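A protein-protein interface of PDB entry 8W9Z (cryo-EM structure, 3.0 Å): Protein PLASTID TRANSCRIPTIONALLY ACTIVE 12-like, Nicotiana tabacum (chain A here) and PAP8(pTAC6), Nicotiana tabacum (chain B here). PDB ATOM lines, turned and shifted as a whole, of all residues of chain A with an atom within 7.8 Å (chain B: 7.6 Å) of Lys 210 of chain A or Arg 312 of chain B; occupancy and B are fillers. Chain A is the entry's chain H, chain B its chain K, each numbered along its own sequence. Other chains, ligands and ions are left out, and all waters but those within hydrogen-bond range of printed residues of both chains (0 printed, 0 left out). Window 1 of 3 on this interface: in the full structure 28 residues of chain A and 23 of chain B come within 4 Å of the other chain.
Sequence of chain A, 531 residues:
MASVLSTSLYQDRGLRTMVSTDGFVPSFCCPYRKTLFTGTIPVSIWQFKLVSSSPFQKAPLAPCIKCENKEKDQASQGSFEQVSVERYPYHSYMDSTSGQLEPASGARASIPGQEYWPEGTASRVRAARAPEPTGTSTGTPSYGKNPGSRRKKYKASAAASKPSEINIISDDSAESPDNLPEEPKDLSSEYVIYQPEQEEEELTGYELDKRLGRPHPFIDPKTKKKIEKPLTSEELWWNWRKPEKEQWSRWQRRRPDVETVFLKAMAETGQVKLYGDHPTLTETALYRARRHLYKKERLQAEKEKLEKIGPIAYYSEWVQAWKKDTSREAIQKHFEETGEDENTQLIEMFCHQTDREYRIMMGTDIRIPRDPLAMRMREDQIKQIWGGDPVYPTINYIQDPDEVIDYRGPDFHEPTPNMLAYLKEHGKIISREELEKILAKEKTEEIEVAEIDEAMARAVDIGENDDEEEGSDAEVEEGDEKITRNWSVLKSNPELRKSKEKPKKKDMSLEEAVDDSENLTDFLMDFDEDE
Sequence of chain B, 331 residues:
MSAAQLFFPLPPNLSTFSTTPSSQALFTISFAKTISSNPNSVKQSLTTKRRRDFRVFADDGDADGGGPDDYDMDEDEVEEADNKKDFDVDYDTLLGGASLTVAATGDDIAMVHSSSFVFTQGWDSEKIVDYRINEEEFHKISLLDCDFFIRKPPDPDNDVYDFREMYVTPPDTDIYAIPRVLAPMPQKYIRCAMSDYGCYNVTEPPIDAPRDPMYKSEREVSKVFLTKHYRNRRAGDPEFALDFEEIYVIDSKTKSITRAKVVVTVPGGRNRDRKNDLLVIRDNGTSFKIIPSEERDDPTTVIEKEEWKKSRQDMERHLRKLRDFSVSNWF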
ATOM      1  N   GLU A 202       5.725  18.642 -13.892  1.00  0.00           N
ATOM      2  CA  GLU A 202       6.024  17.293 -13.428  1.00  0.00           C
ATOM      3  C   GLU A 202       7.395  17.302 -12.762  1.00  0.00           C
ATOM      4  O   GLU A 202       8.406  17.589 -13.411  1.00  0.00           O
ATOM      5  CB  GLU A 202       5.982  16.298 -14.586  1.00  0.00           C
ATOM      6  N   THR A 204       9.005  14.642 -11.281  1.00  0.00           N
ATOM      7  CA  THR A 204       9.785  13.475 -11.668  1.00  0.00           C
ATOM      8  C   THR A 204      10.194  13.564 -13.133  1.00  0.00           C
ATOM      9  O   THR A 204       9.498  14.166 -13.955  1.00  0.00           O
ATOM     10  CB  THR A 204       8.989  12.194 -11.417  1.00  0.00           C
ATOM     11  OG1 THR A 204       9.694  11.074 -11.970  1.00  0.00           O
ATOM     12  CG2 THR A 204       7.612  12.287 -12.052  1.00  0.00           C
ATOM     13  N   GLY A 205      11.340  12.962 -13.455  1.00  0.00           N
ATOM     14  CA  GLY A 205      11.843  13.023 -14.816  1.00  0.00           C
ATOM     15  C   GLY A 205      11.049  12.182 -15.795  1.00  0.00           C
ATOM     16  O   GLY A 205      10.951  12.529 -16.978  1.00  0.00           O
ATOM     17  N   TYR A 206      10.471  11.073 -15.327  1.00  0.00           N
ATOM     18  CA  TYR A 206       9.720  10.196 -16.219  1.00  0.00           C
ATOM     19  C   TYR A 206       8.499  10.905 -16.789  1.00  0.00           C
ATOM     20  O   TYR A 206       8.253  10.864 -18.000  1.00  0.00           O
ATOM     21  CB  TYR A 206       9.305   8.922 -15.483  1.00  0.00           C
ATOM     22  CG  TYR A 206       8.413   8.015 -16.301  1.00  0.00           C
ATOM     23  CD1 TYR A 206       8.949   7.140 -17.235  1.00  0.00           C
ATOM     24  CD2 TYR A 206       7.034   8.033 -16.139  1.00  0.00           C
ATOM     25  CE1 TYR A 206       8.138   6.313 -17.985  1.00  0.00           C
ATOM     26  CE2 TYR A 206       6.216   7.209 -16.884  1.00  0.00           C
ATOM     27  CZ  TYR A 206       6.773   6.351 -17.805  1.00  0.00           C
ATOM     28  OH  TYR A 206       5.960   5.528 -18.549  1.00  0.00           O
ATOM     29  N   GLU A 207       7.717  11.559 -15.929  1.00  0.00           N
ATOM     30  CA  GLU A 207       6.526  12.253 -16.407  1.00  0.00           C
ATOM     31  C   GLU A 207       6.883  13.432 -17.299  1.00  0.00           C
ATOM     32  O   GLU A 207       6.168  13.712 -18.268  1.00  0.00           O
ATOM     33  CB  GLU A 207       5.671  12.710 -15.225  1.00  0.00           C
ATOM     34  CG  GLU A 207       4.998  11.574 -14.469  1.00  0.00           C
ATOM     35  CD  GLU A 207       3.943  10.862 -15.294  1.00  0.00           C
ATOM     36  OE1 GLU A 207       3.403  11.478 -16.237  1.00  0.00           O
ATOM     37  OE2 GLU A 207       3.653   9.684 -14.999  1.00  0.00           O
ATOM     38  N   LEU A 208       7.985  14.125 -17.006  1.00  0.00           N
ATOM     39  CA  LEU A 208       8.414  15.219 -17.871  1.00  0.00           C
ATOM     40  C   LEU A 208       8.809  14.708 -19.251  1.00  0.00           C
ATOM     41  O   LEU A 208       8.422  15.292 -20.270  1.00  0.00           O
ATOM     42  CB  LEU A 208       9.570  15.978 -17.221  1.00  0.00           C
ATOM     43  CG  LEU A 208      10.126  17.190 -17.970  1.00  0.00           C
ATOM     44  CD1 LEU A 208      10.349  18.348 -17.009  1.00  0.00           C
ATOM     45  CD2 LEU A 208      11.422  16.838 -18.683  1.00  0.00           C
ATOM     46  N   ASP A 209       9.572  13.612 -19.303  1.00  0.00           N
ATOM     47  CA  ASP A 209       9.953  13.043 -20.592  1.00  0.00           C
ATOM     48  C   ASP A 209       8.752  12.473 -21.333  1.00  0.00           C
ATOM     49  O   ASP A 209       8.744  12.446 -22.568  1.00  0.00           O
ATOM     50  CB  ASP A 209      11.014  11.961 -20.395  1.00  0.00           C
ATOM     51  CG  ASP A 209      12.285  12.499 -19.772  1.00  0.00           C
ATOM     52  OD1 ASP A 209      12.344  13.715 -19.495  1.00  0.00           O
ATOM     53  OD2 ASP A 209      13.226  11.706 -19.558  1.00  0.00           O
ATOM     54  N   LYS A 210       7.732  12.016 -20.603  1.00  0.00           N
ATOM     55  CA  LYS A 210       6.534  11.502 -21.256  1.00  0.00           C
ATOM     56  C   LYS A 210       5.683  12.636 -21.816  1.00  0.00           C
ATOM     57  O   LYS A 210       5.080  12.497 -22.886  1.00  0.00           O
ATOM     58  CB  LYS A 210       5.726  10.655 -20.273  1.00  0.00           C
ATOM     59  CG  LYS A 210       4.494  10.005 -20.877  1.00  0.00           C
ATOM     60  CD  LYS A 210       3.814   9.081 -19.884  1.00  0.00           C
ATOM     61  CE  LYS A 210       2.609   8.395 -20.505  1.00  0.00           C
ATOM     62  NZ  LYS A 210       1.595   9.378 -20.977  1.00  0.00           N
ATOM     63  N   ARG A 211       5.623  13.766 -21.110  1.00  0.00           N
ATOM     64  CA  ARG A 211       4.848  14.899 -21.604  1.00  0.00           C
ATOM     65  C   ARG A 211       5.544  15.580 -22.775  1.00  0.00           C
ATOM     66  O   ARG A 211       4.892  15.961 -23.754  1.00  0.00           O
ATOM     67  CB  ARG A 211       4.592  15.897 -20.475  1.00  0.00           C
ATOM     68  CG  ARG A 211       3.654  15.387 -19.395  1.00  0.00           C
ATOM     69  CD  ARG A 211       3.400  16.438 -18.323  1.00  0.00           C
ATOM     70  NE  ARG A 211       2.675  17.597 -18.839  1.00  0.00           N
ATOM     71  CZ  ARG A 211       3.243  18.754 -19.163  1.00  0.00           C
ATOM     72  NH1 ARG A 211       2.503  19.752 -19.625  1.00  0.00           N
ATOM     73  NH2 ARG A 211       4.552  18.915 -19.023  1.00  0.00           N
ATOM     74  N   LEU A 212       6.866  15.744 -22.697  1.00  0.00           N
ATOM     75  CA  LEU A 212       7.587  16.400 -23.783  1.00  0.00           C
ATOM     76  C   LEU A 212       7.753  15.479 -24.986  1.00  0.00           C
ATOM     77  O   LEU A 212       7.689  15.936 -26.133  1.00  0.00           O
ATOM     78  CB  LEU A 212       8.952  16.884 -23.296  1.00  0.00           C
ATOM     79  CG  LEU A 212       8.951  17.908 -22.160  1.00  0.00           C
ATOM     80  CD1 LEU A 212      10.363  18.400 -21.885  1.00  0.00           C
ATOM     81  CD2 LEU A 212       8.025  19.069 -22.479  1.00  0.00           C
ATOM     82  N   GLY A 213       7.965  14.188 -24.750  1.00  0.00           N
ATOM     83  CA  GLY A 213       8.188  13.234 -25.813  1.00  0.00           C
ATOM     84  C   GLY A 213       9.610  12.736 -25.947  1.00  0.00           C
ATOM     85  O   GLY A 213       9.940  12.130 -26.973  1.00  0.00           O
ATOM     86  N   ARG A 214      10.460  12.971 -24.951  1.00  0.00           N
ATOM     87  CA  ARG A 214      11.843  12.538 -25.013  1.00  0.00           C
ATOM     88  C   ARG A 214      11.930  11.022 -24.839  1.00  0.00           C
ATOM     89  O   ARG A 214      10.975  10.386 -24.388  1.00  0.00           O
ATOM     90  CB  ARG A 214      12.658  13.254 -23.938  1.00  0.00           C
ATOM     91  CG  ARG A 214      12.500  14.765 -23.961  1.00  0.00           C
ATOM     92  CD  ARG A 214      13.395  15.437 -22.934  1.00  0.00           C
ATOM     93  NE  ARG A 214      14.803  15.369 -23.309  1.00  0.00           N
ATOM     94  CZ  ARG A 214      15.430  16.298 -24.024  1.00  0.00           C
ATOM     95  NH1 ARG A 214      14.773  17.370 -24.442  1.00  0.00           N
ATOM     96  NH2 ARG A 214      16.715  16.155 -24.319  1.00  0.00           N
ATOM     97  N   PRO A 215      13.060  10.417 -25.214  1.00  0.00           N
ATOM     98  CA  PRO A 215      13.215   8.964 -25.034  1.00  0.00           C
ATOM     99  C   PRO A 215      13.019   8.551 -23.583  1.00  0.00           C
ATOM    100  O   PRO A 215      13.698   9.042 -22.679  1.00  0.00           O
ATOM    101  CB  PRO A 215      14.648   8.705 -25.510  1.00  0.00           C
ATOM    102  CG  PRO A 215      14.904   9.780 -26.497  1.00  0.00           C
ATOM    103  CD  PRO A 215      14.176  10.992 -25.987  1.00  0.00           C
ATOM    104  N   HIS A 216      12.075   7.638 -23.368  1.00  0.00           N
ATOM    105  CA  HIS A 216      11.720   7.164 -22.041  1.00  0.00           C
ATOM    106  C   HIS A 216      11.152   5.761 -22.169  1.00  0.00           C
ATOM    107  O   HIS A 216      10.568   5.425 -23.207  1.00  0.00           O
ATOM    108  CB  HIS A 216      10.691   8.085 -21.373  1.00  0.00           C
ATOM    109  CG  HIS A 216       9.294   7.879 -21.865  1.00  0.00           C
ATOM    110  ND1 HIS A 216       8.957   7.955 -23.199  1.00  0.00           N
ATOM    111  CD2 HIS A 216       8.147   7.596 -21.204  1.00  0.00           C
ATOM    112  CE1 HIS A 216       7.664   7.726 -23.338  1.00  0.00           C
ATOM    113  NE2 HIS A 216       7.149   7.507 -22.144  1.00  0.00           N
ATOM    114  N   PRO A 217      11.302   4.921 -21.147  1.00  0.00           N
ATOM    115  CA  PRO A 217      10.719   3.578 -21.211  1.00  0.00           C
ATOM    116  C   PRO A 217       9.201   3.629 -21.200  1.00  0.00           C
ATOM    117  O   PRO A 217       8.589   4.562 -20.676  1.00  0.00           O
ATOM    118  CB  PRO A 217      11.263   2.894 -19.953  1.00  0.00           C
ATOM    119  CG  PRO A 217      11.583   4.013 -19.026  1.00  0.00           C
ATOM    120  CD  PRO A 217      12.052   5.136 -19.899  1.00  0.00           C
ATOM    121  N   PHE A 218       8.591   2.602 -21.797  1.00  0.00           N
ATOM    122  CA  PHE A 218       7.134   2.551 -21.866  1.00  0.00           C
ATOM    123  C   PHE A 218       6.519   2.318 -20.492  1.00  0.00           C
ATOM    124  O   PHE A 218       5.487   2.913 -20.161  1.00  0.00           O
ATOM    125  CB  PHE A 218       6.689   1.460 -22.838  1.00  0.00           C
ATOM    126  CG  PHE A 218       6.834   1.838 -24.283  1.00  0.00           C
ATOM    127  CD1 PHE A 218       5.892   2.643 -24.899  1.00  0.00           C
ATOM    128  CD2 PHE A 218       7.906   1.380 -25.029  1.00  0.00           C
ATOM    129  CE1 PHE A 218       6.019   2.991 -26.228  1.00  0.00           C
ATOM    130  CE2 PHE A 218       8.037   1.725 -26.361  1.00  0.00           C
ATOM    131  CZ  PHE A 218       7.092   2.531 -26.959  1.00  0.00           C
ATOM    132  N   ARG A 290       8.112   6.699 -37.445  1.00  0.00           N
ATOM    133  CA  ARG A 290       8.855   7.944 -37.264  1.00  0.00           C
ATOM    134  C   ARG A 290      10.236   7.746 -37.877  1.00  0.00           C
ATOM    135  O   ARG A 290      11.192   7.373 -37.198  1.00  0.00           O
ATOM    136  CB  ARG A 290       8.940   8.311 -35.790  1.00  0.00           C
ATOM    137  CG  ARG A 290       7.651   8.082 -35.029  1.00  0.00           C
ATOM    138  CD  ARG A 290       7.843   8.362 -33.556  1.00  0.00           C
ATOM    139  NE  ARG A 290       8.108   9.773 -33.300  1.00  0.00           N
ATOM    140  CZ  ARG A 290       8.542  10.247 -32.139  1.00  0.00           C
ATOM    141  NH1 ARG A 290       8.754  11.545 -31.987  1.00  0.00           N
ATOM    142  NH2 ARG A 290       8.772   9.420 -31.130  1.00  0.00           N
ATOM    143  N   GLU B 306      -3.579  18.482 -30.133  1.00  0.00           N
ATOM    144  CA  GLU B 306      -4.591  17.442 -29.989  1.00  0.00           C
ATOM    145  C   GLU B 306      -4.293  16.254 -30.896  1.00  0.00           C
ATOM    146  O   GLU B 306      -4.440  15.093 -30.482  1.00  0.00           O
ATOM    147  CB  GLU B 306      -5.978  18.013 -30.278  1.00  0.00           C
ATOM    148  CG  GLU B 306      -7.112  17.039 -30.017  1.00  0.00           C
ATOM    149  CD  GLU B 306      -8.439  17.736 -29.795  1.00  0.00           C
ATOM    150  OE1 GLU B 306      -8.428  18.910 -29.370  1.00  0.00           O
ATOM    151  OE2 GLU B 306      -9.492  17.112 -30.046  1.00  0.00           O
ATOM    152  N   GLU B 307      -3.860  16.521 -32.133  1.00  0.00           N
ATOM    153  CA  GLU B 307      -3.530  15.432 -33.045  1.00  0.00           C
ATOM    154  C   GLU B 307      -2.368  14.601 -32.515  1.00  0.00           C
ATOM    155  O   GLU B 307      -2.395  13.368 -32.590  1.00  0.00           O
ATOM    156  CB  GLU B 307      -3.205  15.987 -34.431  1.00  0.00           C
ATOM    157  CG  GLU B 307      -4.120  15.473 -35.531  1.00  0.00           C
ATOM    158  CD  GLU B 307      -4.000  13.975 -35.742  1.00  0.00           C
ATOM    159  OE1 GLU B 307      -2.913  13.417 -35.480  1.00  0.00           O
ATOM    160  OE2 GLU B 307      -4.995  13.353 -36.171  1.00  0.00           O
ATOM    161  N   TRP B 308      -1.348  15.259 -31.959  1.00  0.00           N
ATOM    162  CA  TRP B 308      -0.198  14.546 -31.418  1.00  0.00           C
ATOM    163  C   TRP B 308      -0.598  13.684 -30.231  1.00  0.00           C
ATOM    164  O   TRP B 308      -0.168  12.529 -30.123  1.00  0.00           O
ATOM    165  CB  TRP B 308       0.883  15.550 -31.017  1.00  0.00           C
ATOM    166  CG  TRP B 308       2.241  14.954 -30.821  1.00  0.00           C
ATOM    167  CD1 TRP B 308       3.213  14.808 -31.765  1.00  0.00           C
ATOM    168  CD2 TRP B 308       2.786  14.440 -29.601  1.00  0.00           C
ATOM    169  NE1 TRP B 308       4.328  14.229 -31.212  1.00  0.00           N
ATOM    170  CE2 TRP B 308       4.091  13.993 -29.883  1.00  0.00           C
ATOM    171  CE3 TRP B 308       2.297  14.311 -28.299  1.00  0.00           C
ATOM    172  CZ2 TRP B 308       4.911  13.426 -28.913  1.00  0.00           C
ATOM    173  CZ3 TRP B 308       3.113  13.749 -27.337  1.00  0.00           C
ATOM    174  CH2 TRP B 308       4.405  13.314 -27.649  1.00  0.00           C
ATOM    175  N   LYS B 309      -1.430  14.221 -29.335  1.00  0.00           N
ATOM    176  CA  LYS B 309      -1.866  13.442 -28.181  1.00  0.00           C
ATOM    177  C   LYS B 309      -2.658  12.213 -28.615  1.00  0.00           C
ATOM    178  O   LYS B 309      -2.399  11.092 -28.152  1.00  0.00           O
ATOM    179  CB  LYS B 309      -2.692  14.318 -27.240  1.00  0.00           C
ATOM    180  CG  LYS B 309      -3.132  13.619 -25.965  1.00  0.00           C
ATOM    181  CD  LYS B 309      -3.887  14.567 -25.048  1.00  0.00           C
ATOM    182  CE  LYS B 309      -5.142  15.104 -25.717  1.00  0.00           C
ATOM    183  NZ  LYS B 309      -6.086  14.011 -26.081  1.00  0.00           N
ATOM    184  N   LYS B 310      -3.626  12.402 -29.520  1.00  0.00           N
ATOM    185  CA  LYS B 310      -4.429  11.272 -29.977  1.00  0.00           C
ATOM    186  C   LYS B 310      -3.574  10.240 -30.705  1.00  0.00           C
ATOM    187  O   LYS B 310      -3.751   9.028 -30.513  1.00  0.00           O
ATOM    188  CB  LYS B 310      -5.564  11.758 -30.878  1.00  0.00           C
ATOM    189  CG  LYS B 310      -6.570  12.657 -30.182  1.00  0.00           C
ATOM    190  CD  LYS B 310      -7.814  12.858 -31.034  1.00  0.00           C
ATOM    191  CE  LYS B 310      -7.464  13.378 -32.419  1.00  0.00           C
ATOM    192  NZ  LYS B 310      -6.772  14.695 -32.362  1.00  0.00           N
ATOM    193  N   SER B 311      -2.635  10.698 -31.536  1.00  0.00           N
ATOM    194  CA  SER B 311      -1.793   9.772 -32.282  1.00  0.00           C
ATOM    195  C   SER B 311      -0.882   8.983 -31.354  1.00  0.00           C
ATOM    196  O   SER B 311      -0.662   7.786 -31.567  1.00  0.00           O
ATOM    197  CB  SER B 311      -0.972  10.533 -33.321  1.00  0.00           C
ATOM    198  OG  SER B 311      -0.140  11.497 -32.703  1.00  0.00           O
ATOM    199  N   ARG B 312      -0.351   9.627 -30.313  1.00  0.00           N
ATOM    200  CA  ARG B 312       0.492   8.904 -29.368  1.00  0.00           C
ATOM    201  C   ARG B 312      -0.314   7.877 -28.586  1.00  0.00           C
ATOM    202  O   ARG B 312       0.159   6.757 -28.353  1.00  0.00           O
ATOM    203  CB  ARG B 312       1.181   9.879 -28.418  1.00  0.00           C
ATOM    204  CG  ARG B 312       2.093   9.199 -27.420  1.00  0.00           C
ATOM    205  CD  ARG B 312       2.863  10.212 -26.608  1.00  0.00           C
ATOM    206  NE  ARG B 312       3.754   9.572 -25.646  1.00  0.00           N
ATOM    207  CZ  ARG B 312       4.605  10.232 -24.872  1.00  0.00           C
ATOM    208  NH1 ARG B 312       4.685  11.553 -24.947  1.00  0.00           N
ATOM    209  NH2 ARG B 312       5.378   9.574 -24.022  1.00  0.00           N
ATOM    210  N   GLN B 313      -1.533   8.237 -28.174  1.00  0.00           N
ATOM    211  CA  GLN B 313      -2.380   7.266 -27.488  1.00  0.00           C
ATOM    212  C   GLN B 313      -2.673   6.067 -28.382  1.00  0.00           C
ATOM    213  O   GLN B 313      -2.580   4.914 -27.938  1.00  0.00           O
ATOM    214  CB  GLN B 313      -3.678   7.927 -27.027  1.00  0.00           C
ATOM    215  CG  GLN B 313      -3.489   8.989 -25.956  1.00  0.00           C
ATOM    216  CD  GLN B 313      -2.974   8.418 -24.648  1.00  0.00           C
ATOM    217  OE1 GLN B 313      -2.237   9.079 -23.917  1.00  0.00           O
ATOM    218  NE2 GLN B 313      -3.368   7.187 -24.342  1.00  0.00           N
ATOM    219  N   ASP B 314      -3.006   6.318 -29.651  1.00  0.00           N
ATOM    220  CA  ASP B 314      -3.291   5.220 -30.570  1.00  0.00           C
ATOM    221  C   ASP B 314      -2.055   4.362 -30.816  1.00  0.00           C
ATOM    222  O   ASP B 314      -2.154   3.132 -30.898  1.00  0.00           O
ATOM    223  CB  ASP B 314      -3.836   5.768 -31.889  1.00  0.00           C
ATOM    224  CG  ASP B 314      -5.145   6.511 -31.715  1.00  0.00           C
ATOM    225  OD1 ASP B 314      -5.912   6.157 -30.795  1.00  0.00           O
ATOM    226  OD2 ASP B 314      -5.406   7.449 -32.497  1.00  0.00           O
ATOM    227  N   MET B 315      -0.881   4.988 -30.925  1.00  0.00           N
ATOM    228  CA  MET B 315       0.342   4.229 -31.166  1.00  0.00           C
ATOM    229  C   MET B 315       0.688   3.346 -29.976  1.00  0.00           C
ATOM    230  O   MET B 315       1.084   2.187 -30.152  1.00  0.00           O
ATOM    231  CB  MET B 315       1.496   5.179 -31.479  1.00  0.00           C
ATOM    232  CG  MET B 315       2.744   4.487 -31.996  1.00  0.00           C
ATOM    233  SD  MET B 315       2.476   3.706 -33.598  1.00  0.00           S
ATOM    234  CE  MET B 315       4.084   2.986 -33.905  1.00  0.00           C
ATOM    235  N   GLU B 316       0.548   3.872 -28.757  1.00  0.00           N
ATOM    236  CA  GLU B 316       0.802   3.051 -27.578  1.00  0.00           C
ATOM    237  C   GLU B 316      -0.210   1.918 -27.470  1.00  0.00           C
ATOM    238  O   GLU B 316       0.151   0.788 -27.116  1.00  0.00           O
ATOM    239  CB  GLU B 316       0.787   3.917 -26.319  1.00  0.00           C
ATOM    240  CG  GLU B 316       1.903   4.948 -26.272  1.00  0.00           C
ATOM    241  CD  GLU B 316       1.867   5.797 -25.019  1.00  0.00           C
ATOM    242  OE1 GLU B 316       1.010   5.539 -24.147  1.00  0.00           O
ATOM    243  OE2 GLU B 316       2.695   6.726 -24.904  1.00  0.00           O
ATOM    244  N   ARG B 317      -1.418   2.111 -27.943  1.00  0.00           N
ATOM    245  CA  ARG B 317      -2.370   1.010 -27.928  1.00  0.00           C
ATOM    246  C   ARG B 317      -1.959  -0.085 -28.871  1.00  0.00           C
ATOM    247  O   ARG B 317      -2.024  -1.249 -28.532  1.00  0.00           O
ATOM    248  CB  ARG B 317      -3.742   1.491 -28.323  1.00  0.00           C
ATOM    249  CG  ARG B 317      -4.870   0.556 -27.958  1.00  0.00           C
ATOM    250  CD  ARG B 317      -6.173   1.040 -28.570  1.00  0.00           C
ATOM    251  NE  ARG B 317      -6.233   2.497 -28.672  1.00  0.00           N
ATOM    252  CZ  ARG B 317      -6.670   3.302 -27.709  1.00  0.00           C
ATOM    253  NH1 ARG B 317      -7.077   2.800 -26.552  1.00  0.00           N
ATOM    254  NH2 ARG B 317      -6.692   4.613 -27.899  1.00  0.00           N
ATOM    255  N   HIS B 318      -1.556   0.274 -30.074  1.00  0.00           N
ATOM    256  CA  HIS B 318      -1.199  -0.727 -31.064  1.00  0.00           C
ATOM    257  C   HIS B 318      -0.022  -1.518 -30.623  1.00  0.00           C
ATOM    258  O   HIS B 318       0.016  -2.704 -30.809  1.00  0.00           O
ATOM    259  CB  HIS B 318      -0.877  -0.068 -32.388  1.00  0.00           C
ATOM    260  CG  HIS B 318      -0.413  -1.005 -33.452  1.00  0.00           C
ATOM    261  ND1 HIS B 318      -1.262  -1.874 -34.100  1.00  0.00           N
ATOM    262  CD2 HIS B 318       0.805  -1.178 -34.015  1.00  0.00           C
ATOM    263  CE1 HIS B 318      -0.581  -2.561 -34.999  1.00  0.00           C
ATOM    264  NE2 HIS B 318       0.676  -2.157 -34.969  1.00  0.00           N
ATOM    265  N   TRP B 330      10.511   4.521 -26.025  1.00  0.00           N
ATOM    266  CA  TRP B 330       9.772   5.363 -26.962  1.00  0.00           C
ATOM    267  C   TRP B 330      10.669   6.530 -27.357  1.00  0.00           C
ATOM    268  O   TRP B 330      10.774   7.520 -26.628  1.00  0.00           O
ATOM    269  CB  TRP B 330       8.461   5.849 -26.351  1.00  0.00           C
ATOM    270  CG  TRP B 330       7.514   6.426 -27.361  1.00  0.00           C
ATOM    271  CD1 TRP B 330       6.585   5.747 -28.096  1.00  0.00           C
ATOM    272  CD2 TRP B 330       7.404   7.801 -27.750  1.00  0.00           C
ATOM    273  NE1 TRP B 330       5.904   6.613 -28.915  1.00  0.00           N
ATOM    274  CE2 TRP B 330       6.388   7.879 -28.722  1.00  0.00           C
ATOM    275  CE3 TRP B 330       8.064   8.971 -27.369  1.00  0.00           C
ATOM    276  CZ2 TRP B 330       6.018   9.081 -29.317  1.00  0.00           C
ATOM    277  CZ3 TRP B 330       7.695  10.163 -27.961  1.00  0.00           C
ATOM    278  CH2 TRP B 330       6.681  10.209 -28.924  1.00  0.00           C
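NE2 of His 216 of chain A lies close to NH2 of Arg 312 of chain B. The backbone carbonyl oxygen (O) of Lys 210 of chain A sits close to the guanidinium group (NH2) of Arg 312 of chain B, at 3.2 Å. The backbone NH (N) of Trp 330 of chain B lies within hydrogen-bond range of the backbone carbonyl oxygen (O) of His 216 of chain A (3.0 Å).
O of Asp 209 of chain A is in hydrogen-bond range of N of Arg 214 of chain A. The guanidinium group (NE) of Arg 312 of chain B is in salt-bridge range of the side-chain carboxylate (OE2) of Glu 316 of chain B (3.1 Å). The side-chain hydroxyl of Tyr 206 of chain A sits at hydrogen-bond distance from the backbone carbonyl oxygen of Phe 218 of chain A (3.1 Å). The backbone carbonyl oxygen (O) of Arg 214 of chain A is in hydrogen-bond range of a ring nitrogen (ND1) of His 216 of chain A (3.4 Å).
Among the printed residues, pairs that only touch across the chains: Gly 213 of chain A with Arg 312 of chain B (3.98 Å), Gly 213 of chain A with Trp 330 of chain B (3.1 Å), Arg 214 of chain A with Trp 330 of chain B (3.6 Å), Pro 215 of chain A with Trp 330 of chain B (3.3 Å), Phe 218 of chain A with Trp 330 of chain B (3.4 Å) and Arg 290 of chain A with Trp 330 of chain B (3.1 Å).
Of chain B, only Arg 312 (2.3 Å) comes within 4 Å of Lys 210 of chain A. No residue of chain A comes within 4 Å of Ser 311 of chain B. Printed residues of chain A within 4 Å of Trp 330 of chain B: Gly 213 (3.1 Å), Arg 214 (3.6 Å), Pro 215 (3.3 Å), His 216 (3.0 Å), Phe 218 (3.4 Å) and Arg 290 (3.1 Å). Of the printed residues of chain B, Pro 215 of chain A touches Trp 330. Of the printed residues of chain B, Arg 290 of chain A touches Trp 330. The nearest residue of chain B that does not touch Lys 210 of chain A is Glu 316 of chain B (4.7 Å).
Of the 14 printed residues of chain B, 2 touch a printed residue of chain A. Hydrophobic or aromatic side chains of chain B that line the printed part of chain A: Trp 330. Among the printed residues, no Asp or Glu carboxylate lies within 4 Å of a Lys or Arg side-chain nitrogen of the other chain.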
